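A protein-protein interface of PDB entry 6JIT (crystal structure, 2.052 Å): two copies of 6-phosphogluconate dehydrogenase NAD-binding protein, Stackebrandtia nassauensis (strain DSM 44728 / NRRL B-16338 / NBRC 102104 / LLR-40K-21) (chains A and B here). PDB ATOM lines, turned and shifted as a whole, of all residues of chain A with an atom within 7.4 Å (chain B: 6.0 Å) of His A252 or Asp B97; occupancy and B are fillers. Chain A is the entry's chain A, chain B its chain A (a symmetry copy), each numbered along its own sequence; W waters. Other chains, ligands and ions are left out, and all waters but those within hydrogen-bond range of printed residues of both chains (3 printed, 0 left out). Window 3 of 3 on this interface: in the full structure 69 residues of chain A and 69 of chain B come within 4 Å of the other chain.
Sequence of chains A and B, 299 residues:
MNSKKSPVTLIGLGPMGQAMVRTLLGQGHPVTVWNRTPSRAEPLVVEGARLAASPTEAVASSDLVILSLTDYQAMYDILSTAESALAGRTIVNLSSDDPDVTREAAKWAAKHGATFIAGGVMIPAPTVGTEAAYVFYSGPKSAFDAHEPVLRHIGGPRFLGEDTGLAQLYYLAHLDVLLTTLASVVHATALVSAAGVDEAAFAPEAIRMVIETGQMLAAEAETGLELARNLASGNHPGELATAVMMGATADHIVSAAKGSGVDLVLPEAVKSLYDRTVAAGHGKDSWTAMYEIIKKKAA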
ATOM      1  N   LEU A 191     -16.732  20.684 -16.493  1.00  0.00           N
ATOM      2  CA  LEU A 191     -16.213  19.322 -16.423  1.00  0.00           C
ATOM      3  C   LEU A 191     -14.762  19.314 -15.952  1.00  0.00           C
ATOM      4  O   LEU A 191     -14.387  18.533 -15.070  1.00  0.00           O
ATOM      5  CB  LEU A 191     -16.351  18.659 -17.794  1.00  0.00           C
ATOM      6  CG  LEU A 191     -16.036  17.175 -17.942  1.00  0.00           C
ATOM      7  CD1 LEU A 191     -17.011  16.339 -17.130  1.00  0.00           C
ATOM      8  CD2 LEU A 191     -16.083  16.790 -19.414  1.00  0.00           C
ATOM      9  N   MET A 245     -18.311   5.021 -33.053  1.00  0.00           N
ATOM     10  CA  MET A 245     -17.138   5.617 -32.422  1.00  0.00           C
ATOM     11  C   MET A 245     -17.507   6.882 -31.658  1.00  0.00           C
ATOM     12  O   MET A 245     -17.075   7.078 -30.516  1.00  0.00           O
ATOM     13  CB  MET A 245     -16.070   5.926 -33.471  1.00  0.00           C
ATOM     14  CG  MET A 245     -15.555   4.722 -34.226  1.00  0.00           C
ATOM     15  SD  MET A 245     -14.344   5.186 -35.479  1.00  0.00           S
ATOM     16  CE  MET A 245     -12.815   4.816 -34.624  1.00  0.00           C
ATOM     17  N   MET A 246     -18.296   7.764 -32.279  1.00  0.00           N
ATOM     18  CA  MET A 246     -18.718   8.981 -31.591  1.00  0.00           C
ATOM     19  C   MET A 246     -19.620   8.661 -30.410  1.00  0.00           C
ATOM     20  O   MET A 246     -19.564   9.337 -29.376  1.00  0.00           O
ATOM     21  CB  MET A 246     -19.447   9.916 -32.549  1.00  0.00           C
ATOM     22  CG  MET A 246     -18.679  10.306 -33.785  1.00  0.00           C
ATOM     23  SD  MET A 246     -17.327  11.458 -33.511  1.00  0.00           S
ATOM     24  CE  MET A 246     -17.290  12.261 -35.112  1.00  0.00           C
ATOM     25  N   GLY A 247     -20.485   7.656 -30.559  1.00  0.00           N
ATOM     26  CA  GLY A 247     -21.353   7.272 -29.459  1.00  0.00           C
ATOM     27  C   GLY A 247     -20.577   6.830 -28.234  1.00  0.00           C
ATOM     28  O   GLY A 247     -20.972   7.117 -27.101  1.00  0.00           O
ATOM     29  N   ALA A 248     -19.456   6.130 -28.442  1.00  0.00           N
ATOM     30  CA  ALA A 248     -18.636   5.712 -27.309  1.00  0.00           C
ATOM     31  C   ALA A 248     -18.005   6.914 -26.618  1.00  0.00           C
ATOM     32  O   ALA A 248     -17.887   6.939 -25.389  1.00  0.00           O
ATOM     33  CB  ALA A 248     -17.561   4.727 -27.767  1.00  0.00           C
ATOM     34  N   THR A 249     -17.601   7.920 -27.392  1.00  0.00           N
ATOM     35  CA  THR A 249     -17.070   9.139 -26.794  1.00  0.00           C
ATOM     36  C   THR A 249     -18.155   9.892 -26.035  1.00  0.00           C
ATOM     37  O   THR A 249     -17.918  10.381 -24.923  1.00  0.00           O
ATOM     38  CB  THR A 249     -16.452  10.025 -27.875  1.00  0.00           C
ATOM     39  OG1 THR A 249     -15.422   9.293 -28.551  1.00  0.00           O
ATOM     40  CG2 THR A 249     -15.852  11.279 -27.261  1.00  0.00           C
ATOM     41  N   ALA A 250     -19.357   9.981 -26.612  1.00  0.00           N
ATOM     42  CA  ALA A 250     -20.475  10.590 -25.902  1.00  0.00           C
ATOM     43  C   ALA A 250     -20.758   9.859 -24.594  1.00  0.00           C
ATOM     44  O   ALA A 250     -21.033  10.492 -23.567  1.00  0.00           O
ATOM     45  CB  ALA A 250     -21.715  10.606 -26.795  1.00  0.00           C
ATOM     46  N   ASP A 251     -20.683   8.524 -24.610  1.00  0.00           N
ATOM     47  CA  ASP A 251     -20.868   7.758 -23.381  1.00  0.00           C
ATOM     48  C   ASP A 251     -19.811   8.116 -22.343  1.00  0.00           C
ATOM     49  O   ASP A 251     -20.121   8.250 -21.153  1.00  0.00           O
ATOM     50  CB  ASP A 251     -20.835   6.259 -23.684  1.00  0.00           C
ATOM     51  CG  ASP A 251     -22.018   5.799 -24.520  1.00  0.00           C
ATOM     52  OD1 ASP A 251     -22.960   6.594 -24.724  1.00  0.00           O
ATOM     53  OD2 ASP A 251     -22.006   4.638 -24.975  1.00  0.00           O
ATOM     54  N   HIS A 252     -18.555   8.280 -22.775  1.00  0.00           N
ATOM     55  CA  HIS A 252     -17.493   8.631 -21.834  1.00  0.00           C
ATOM     56  C   HIS A 252     -17.706  10.022 -21.251  1.00  0.00           C
ATOM     57  O   HIS A 252     -17.459  10.246 -20.060  1.00  0.00           O
ATOM     58  CB  HIS A 252     -16.127   8.547 -22.517  1.00  0.00           C
ATOM     59  CG  HIS A 252     -15.751   7.165 -22.957  1.00  0.00           C
ATOM     60  ND1 HIS A 252     -16.194   6.031 -22.312  1.00  0.00           N
ATOM     61  CD2 HIS A 252     -14.971   6.739 -23.978  1.00  0.00           C
ATOM     62  CE1 HIS A 252     -15.702   4.964 -22.916  1.00  0.00           C
ATOM     63  NE2 HIS A 252     -14.959   5.366 -23.932  1.00  0.00           N
ATOM     64  N   ILE A 253     -18.157  10.970 -22.078  1.00  0.00           N
ATOM     65  CA  ILE A 253     -18.430  12.318 -21.586  1.00  0.00           C
ATOM     66  C   ILE A 253     -19.510  12.281 -20.512  1.00  0.00           C
ATOM     67  O   ILE A 253     -19.412  12.967 -19.486  1.00  0.00           O
ATOM     68  CB  ILE A 253     -18.816  13.243 -22.755  1.00  0.00           C
ATOM     69  CG1 ILE A 253     -17.638  13.405 -23.722  1.00  0.00           C
ATOM     70  CG2 ILE A 253     -19.282  14.602 -22.241  1.00  0.00           C
ATOM     71  CD1 ILE A 253     -18.023  14.007 -25.061  1.00  0.00           C
ATOM     72  N   VAL A 254     -20.543  11.459 -20.719  1.00  0.00           N
ATOM     73  CA  VAL A 254     -21.612  11.333 -19.729  1.00  0.00           C
ATOM     74  C   VAL A 254     -21.072  10.740 -18.433  1.00  0.00           C
ATOM     75  O   VAL A 254     -21.338  11.253 -17.338  1.00  0.00           O
ATOM     76  CB  VAL A 254     -22.772  10.491 -20.294  1.00  0.00           C
ATOM     77  CG1 VAL A 254     -23.752  10.119 -19.185  1.00  0.00           C
ATOM     78  CG2 VAL A 254     -23.484  11.250 -21.407  1.00  0.00           C
ATOM     79  N   SER A 255     -20.308   9.647 -18.535  1.00  0.00           N
ATOM     80  CA  SER A 255     -19.781   9.017 -17.328  1.00  0.00           C
ATOM     81  C   SER A 255     -18.813   9.947 -16.605  1.00  0.00           C
ATOM     82  O   SER A 255     -18.820  10.024 -15.371  1.00  0.00           O
ATOM     83  CB  SER A 255     -19.112   7.680 -17.668  1.00  0.00           C
ATOM     84  OG  SER A 255     -17.926   7.859 -18.422  1.00  0.00           O
ATOM     85  N   ALA A 256     -17.994  10.685 -17.360  1.00  0.00           N
ATOM     86  CA  ALA A 256     -17.120  11.685 -16.751  1.00  0.00           C
ATOM     87  C   ALA A 256     -17.928  12.758 -16.029  1.00  0.00           C
ATOM     88  O   ALA A 256     -17.617  13.124 -14.890  1.00  0.00           O
ATOM     89  CB  ALA A 256     -16.220  12.315 -17.816  1.00  0.00           C
ATOM     90  N   ALA A 257     -18.975  13.275 -16.677  1.00  0.00           N
ATOM     91  CA  ALA A 257     -19.802  14.295 -16.037  1.00  0.00           C
ATOM     92  C   ALA A 257     -20.548  13.726 -14.839  1.00  0.00           C
ATOM     93  O   ALA A 257     -20.695  14.400 -13.812  1.00  0.00           O
ATOM     94  CB  ALA A 257     -20.781  14.896 -17.045  1.00  0.00           C
ATOM     95  N   LYS A 258     -21.021  12.483 -14.951  1.00  0.00           N
ATOM     96  CA  LYS A 258     -21.697  11.836 -13.833  1.00  0.00           C
ATOM     97  C   LYS A 258     -20.760  11.642 -12.649  1.00  0.00           C
ATOM     98  O   LYS A 258     -21.195  11.731 -11.495  1.00  0.00           O
ATOM     99  CB  LYS A 258     -22.278  10.495 -14.286  1.00  0.00           C
ATOM    100  CG  LYS A 258     -23.491  10.037 -13.501  1.00  0.00           C
ATOM    101  CD  LYS A 258     -24.006   8.703 -14.021  1.00  0.00           C
ATOM    102  CE  LYS A 258     -24.364   8.780 -15.497  1.00  0.00           C
ATOM    103  NZ  LYS A 258     -24.814   7.462 -16.029  1.00  0.00           N
ATOM    104  N   LYS A 271     -25.671  11.933 -26.119  1.00  0.00           N
ATOM    105  CA  LYS A 271     -25.650  10.477 -26.003  1.00  0.00           C
ATOM    106  C   LYS A 271     -26.951   9.868 -26.507  1.00  0.00           C
ATOM    107  O   LYS A 271     -26.944   8.804 -27.138  1.00  0.00           O
ATOM    108  CB  LYS A 271     -25.386  10.074 -24.551  1.00  0.00           C
ATOM    109  CG  LYS A 271     -25.585   8.591 -24.249  1.00  0.00           C
ATOM    110  CD  LYS A 271     -25.225   8.276 -22.799  1.00  0.00           C
ATOM    111  CE  LYS A 271     -25.873   6.981 -22.315  1.00  0.00           C
ATOM    112  NZ  LYS A 271     -25.579   5.833 -23.212  1.00  0.00           N
ATOM    113  N   THR B  70      -9.132   0.773 -28.572  1.00  0.00           N
ATOM    114  CA  THR B  70     -10.464   1.369 -28.553  1.00  0.00           C
ATOM    115  C   THR B  70     -10.832   1.873 -27.163  1.00  0.00           C
ATOM    116  O   THR B  70     -11.477   2.918 -27.028  1.00  0.00           O
ATOM    117  CB  THR B  70     -11.504   0.361 -29.047  1.00  0.00           C
ATOM    118  OG1 THR B  70     -11.584  -0.738 -28.130  1.00  0.00           O
ATOM    119  CG2 THR B  70     -11.131  -0.159 -30.425  1.00  0.00           C
ATOM    120  N   ASP B  71     -10.429   1.153 -26.120  1.00  0.00           N
ATOM    121  CA  ASP B  71     -10.716   1.573 -24.753  1.00  0.00           C
ATOM    122  C   ASP B  71      -9.755   0.861 -23.807  1.00  0.00           C
ATOM    123  O   ASP B  71      -8.928   0.044 -24.223  1.00  0.00           O
ATOM    124  CB  ASP B  71     -12.183   1.314 -24.389  1.00  0.00           C
ATOM    125  CG  ASP B  71     -12.592  -0.143 -24.553  1.00  0.00           C
ATOM    126  OD1 ASP B  71     -11.711  -1.027 -24.631  1.00  0.00           O
ATOM    127  OD2 ASP B  71     -13.813  -0.402 -24.607  1.00  0.00           O
ATOM    128  N   TYR B  72      -9.874   1.182 -22.518  1.00  0.00           N
ATOM    129  CA  TYR B  72      -8.952   0.624 -21.534  1.00  0.00           C
ATOM    130  C   TYR B  72      -9.203  -0.859 -21.303  1.00  0.00           C
ATOM    131  O   TYR B  72      -8.276  -1.591 -20.936  1.00  0.00           O
ATOM    132  CB  TYR B  72      -9.051   1.412 -20.227  1.00  0.00           C
ATOM    133  CG  TYR B  72      -8.068   2.558 -20.160  1.00  0.00           C
ATOM    134  CD1 TYR B  72      -7.997   3.498 -21.185  1.00  0.00           C
ATOM    135  CD2 TYR B  72      -7.206   2.698 -19.081  1.00  0.00           C
ATOM    136  CE1 TYR B  72      -7.097   4.542 -21.134  1.00  0.00           C
ATOM    137  CE2 TYR B  72      -6.299   3.748 -19.023  1.00  0.00           C
ATOM    138  CZ  TYR B  72      -6.246   4.661 -20.049  1.00  0.00           C
ATOM    139  OH  TYR B  72      -5.350   5.704 -19.992  1.00  0.00           O
ATOM    140  N   GLN B  73     -10.437  -1.324 -21.521  1.00  0.00           N
ATOM    141  CA  GLN B  73     -10.713  -2.753 -21.431  1.00  0.00           C
ATOM    142  C   GLN B  73      -9.867  -3.545 -22.423  1.00  0.00           C
ATOM    143  O   GLN B  73      -9.435  -4.661 -22.116  1.00  0.00           O
ATOM    144  CB  GLN B  73     -12.201  -3.015 -21.664  1.00  0.00           C
ATOM    145  CG  GLN B  73     -12.619  -4.463 -21.446  1.00  0.00           C
ATOM    146  CD  GLN B  73     -12.335  -4.944 -20.034  1.00  0.00           C
ATOM    147  OE1 GLN B  73     -12.638  -4.256 -19.056  1.00  0.00           O
ATOM    148  NE2 GLN B  73     -11.742  -6.126 -19.921  1.00  0.00           N
ATOM    149  N   SER B  95      -5.389   5.652 -25.341  1.00  0.00           N
ATOM    150  CA  SER B  95      -6.769   5.302 -25.641  1.00  0.00           C
ATOM    151  C   SER B  95      -7.733   6.180 -24.852  1.00  0.00           C
ATOM    152  O   SER B  95      -7.439   6.617 -23.737  1.00  0.00           O
ATOM    153  CB  SER B  95      -7.034   3.831 -25.315  1.00  0.00           C
ATOM    154  OG  SER B  95      -5.915   3.023 -25.650  1.00  0.00           O
ATOM    155  N   SER B  96      -8.902   6.424 -25.436  1.00  0.00           N
ATOM    156  CA  SER B  96      -9.918   7.245 -24.797  1.00  0.00           C
ATOM    157  C   SER B  96     -10.806   6.391 -23.903  1.00  0.00           C
ATOM    158  O   SER B  96     -11.212   5.287 -24.278  1.00  0.00           O
ATOM    159  CB  SER B  96     -10.772   7.968 -25.842  1.00  0.00           C
ATOM    160  OG  SER B  96     -11.665   8.874 -25.219  1.00  0.00           O
ATOM    161  N   ASP B  97     -11.102   6.909 -22.713  1.00  0.00           N
ATOM    162  CA  ASP B  97     -11.971   6.218 -21.764  1.00  0.00           C
ATOM    163  C   ASP B  97     -12.337   7.194 -20.650  1.00  0.00           C
ATOM    164  O   ASP B  97     -11.837   8.323 -20.591  1.00  0.00           O
ATOM    165  CB  ASP B  97     -11.307   4.954 -21.204  1.00  0.00           C
ATOM    166  CG  ASP B  97     -12.312   3.849 -20.911  1.00  0.00           C
ATOM    167  OD1 ASP B  97     -13.394   4.155 -20.366  1.00  0.00           O
ATOM    168  OD2 ASP B  97     -12.028   2.678 -21.242  1.00  0.00           O
ATOM    169  N   ASP B  98     -13.224   6.744 -19.768  1.00  0.00           N
ATOM    170  CA  ASP B  98     -13.647   7.547 -18.630  1.00  0.00           C
ATOM    171  C   ASP B  98     -12.444   7.889 -17.751  1.00  0.00           C
ATOM    172  O   ASP B  98     -11.553   7.050 -17.565  1.00  0.00           O
ATOM    173  CB  ASP B  98     -14.701   6.780 -17.829  1.00  0.00           C
ATOM    174  CG  ASP B  98     -15.045   7.446 -16.516  1.00  0.00           C
ATOM    175  OD1 ASP B  98     -15.841   8.407 -16.520  1.00  0.00           O
ATOM    176  OD2 ASP B  98     -14.524   7.001 -15.472  1.00  0.00           O
ATOM    177  N   PRO B  99     -12.372   9.113 -17.210  1.00  0.00           N
ATOM    178  CA  PRO B  99     -11.185   9.484 -16.417  1.00  0.00           C
ATOM    179  C   PRO B  99     -10.967   8.615 -15.192  1.00  0.00           C
ATOM    180  O   PRO B  99      -9.819   8.281 -14.878  1.00  0.00           O
ATOM    181  CB  PRO B  99     -11.464  10.946 -16.037  1.00  0.00           C
ATOM    182  CG  PRO B  99     -12.388  11.440 -17.111  1.00  0.00           C
ATOM    183  CD  PRO B  99     -13.261  10.263 -17.448  1.00  0.00           C
ATOM    184  N   VAL B 101     -11.790   5.534 -14.966  1.00  0.00           N
ATOM    185  CA  VAL B 101     -11.269   4.275 -15.488  1.00  0.00           C
ATOM    186  C   VAL B 101      -9.759   4.361 -15.664  1.00  0.00           C
ATOM    187  O   VAL B 101      -9.025   3.425 -15.322  1.00  0.00           O
ATOM    188  CB  VAL B 101     -11.976   3.901 -16.805  1.00  0.00           C
ATOM    189  CG1 VAL B 101     -11.260   2.741 -17.488  1.00  0.00           C
ATOM    190  CG2 VAL B 101     -13.436   3.547 -16.545  1.00  0.00           C
ATOM    191  N   THR B 102      -9.265   5.489 -16.186  1.00  0.00           N
ATOM    192  CA  THR B 102      -7.823   5.634 -16.355  1.00  0.00           C
ATOM    193  C   THR B 102      -7.110   5.702 -15.009  1.00  0.00           C
ATOM    194  O   THR B 102      -5.986   5.203 -14.882  1.00  0.00           O
ATOM    195  CB  THR B 102      -7.493   6.870 -17.200  1.00  0.00           C
ATOM    196  OG1 THR B 102      -7.737   8.063 -16.445  1.00  0.00           O
ATOM    197  CG2 THR B 102      -8.333   6.896 -18.474  1.00  0.00           C
ATOM    198  N   GLN B 168      -7.516  12.383 -20.022  1.00  0.00           N
ATOM    199  CA  GLN B 168      -8.799  12.039 -20.618  1.00  0.00           C
ATOM    200  C   GLN B 168      -9.900  13.004 -20.198  1.00  0.00           C
ATOM    201  O   GLN B 168     -10.860  13.200 -20.951  1.00  0.00           O
ATOM    202  CB  GLN B 168      -9.178  10.598 -20.275  1.00  0.00           C
ATOM    203  CG  GLN B 168      -8.445   9.575 -21.140  1.00  0.00           C
ATOM    204  CD  GLN B 168      -8.681   9.805 -22.622  1.00  0.00           C
ATOM    205  OE1 GLN B 168      -9.823   9.935 -23.064  1.00  0.00           O
ATOM    206  NE2 GLN B 168      -7.600   9.876 -23.394  1.00  0.00           N
ATOM    207  N   LEU B 169      -9.781  13.621 -19.021  1.00  0.00           N
ATOM    208  CA  LEU B 169     -10.730  14.666 -18.643  1.00  0.00           C
ATOM    209  C   LEU B 169     -10.661  15.842 -19.613  1.00  0.00           C
ATOM    210  O   LEU B 169     -11.691  16.312 -20.109  1.00  0.00           O
ATOM    211  CB  LEU B 169     -10.462  15.127 -17.210  1.00  0.00           C
ATOM    212  CG  LEU B 169     -11.352  16.268 -16.709  1.00  0.00           C
ATOM    213  CD1 LEU B 169     -12.812  15.845 -16.696  1.00  0.00           C
ATOM    214  CD2 LEU B 169     -10.910  16.717 -15.325  1.00  0.00           C
ATOM    215  N   LEU B 172     -11.899  14.609 -23.155  1.00  0.00           N
ATOM    216  CA  LEU B 172     -13.349  14.468 -23.246  1.00  0.00           C
ATOM    217  C   LEU B 172     -14.057  15.817 -23.181  1.00  0.00           C
ATOM    218  O   LEU B 172     -15.119  15.987 -23.789  1.00  0.00           O
ATOM    219  CB  LEU B 172     -13.855  13.539 -22.139  1.00  0.00           C
ATOM    220  CG  LEU B 172     -13.438  12.064 -22.247  1.00  0.00           C
ATOM    221  CD1 LEU B 172     -13.881  11.274 -21.019  1.00  0.00           C
ATOM    222  CD2 LEU B 172     -13.981  11.431 -23.520  1.00  0.00           C
HETATM  223  O   HOH W   1     -15.510   2.418 -25.710  1.00  0.00           O
HETATM  224  O   HOH W   2     -13.521   4.367 -26.019  1.00  0.00           O
HETATM  225  O   HOH W   3     -12.488   9.126 -28.489  1.00  0.00           O
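Among the printed residues, pairs that only touch across the chains: Leu A191 with Leu B169, His A252 with Asp B97, Ile A253 with Leu B172, Ala A256 with Pro B99, His A252 with Leu B172, His A252 with Ser B96 and His A252 with Asp B98.
The side-chain carboxylate (OD2) of Asp B98 sits at hydrogen-bond distance from the backbone NH (N) of Val B101, at 3.1 Å. OG of Ser B96 is in hydrogen-bond range of OE1 of Gln B168, 3.0 Å away. The backbone carbonyl oxygen (O) of His A252 sits at hydrogen-bond distance from the side-chain hydroxyl (OG) of Ser A255, at 2.9 Å. The backbone carbonyl oxygen of Pro B99 sits at hydrogen-bond distance from the side-chain hydroxyl of Thr B102. The side-chain carboxylate of Asp B97 lies within hydrogen-bond range of the backbone NH of Tyr B72. The backbone NH of Asp B97 lies within hydrogen-bond range of the side-chain amide oxygen of Gln B168 (3.3 Å).
Hydrophobic or aromatic side chains of chain A within 4 Å of the printed part of chain B: Leu A191, His A252, Ile A253 and Ala A256. Printed residues of chain B that touch a printed residue of chain A: Ser B96, Asp B97, Asp B98, Pro B99, Leu B169 and Leu B172. Hydrophobic or aromatic side chains of chain B that line the printed part of chain A: Pro B99, Leu B169 and Leu B172. Among the printed residues, no Asp or Glu carboxylate lies within 4 Å of a Lys or Arg side-chain nitrogen of the other chain.
No position is printed for both chains. Of the 9 pairs that touch across the chains among the printed residues, none has its exchanged pair printed and touching as well.
The backbone NH of Ala A256 sits at hydrogen-bond distance from the side-chain carboxylate of Asp B98, at 3.2 Å. The side-chain hydroxyl (OG) of Ser A255 lies within hydrogen-bond range of the side-chain carboxylate (OD1) of Asp B98, at 2.9 Å.
Of the printed residues of chain B, His A252 touches Ser B96, Asp B97, Asp B98 and Leu B172. Asp B97 touches just one residue of chain A: His A252 (3.5 Å). Of the printed residues of chain B, Leu A191 touches Leu B169 (3.5 Å). Of the printed residues of chain A, Ser B96 touches His A252. Printed residues of chain A within 4 Å of Pro B99: Ala A256. Of the printed residues of chain A, Leu B172 touches His A252 and Ile A253. Of the printed residues of chain A, Leu B169 touches Leu A191 (3.5 Å). Val B101 touches none of the printed residues of chain A. Lys A271 touches none of the printed residues of chain B. The nearest printed residue of chain B that does not touch His A252 is Asp B71 (4.9 Å). The nearest printed residue of chain A that does not touch Leu B172 is Ala A256 (4.1 Å).
Water W2 lies within hydrogen-bond range of the backbone carbonyl oxygen of Thr B70 (2.7 Å), a ring nitrogen (NE2) of His A252 (2.7 Å) and the backbone carbonyl oxygen of Ser B96 (3.0 Å). Water W3 lies within hydrogen-bond range of OG1 of Thr A249 (2.9 Å) and OG of Ser B96 (3.4 Å). Water W1 lies within hydrogen-bond range of the side-chain carboxylate (OD2) of Asp B71 and a ring nitrogen (NE2) of His A252.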
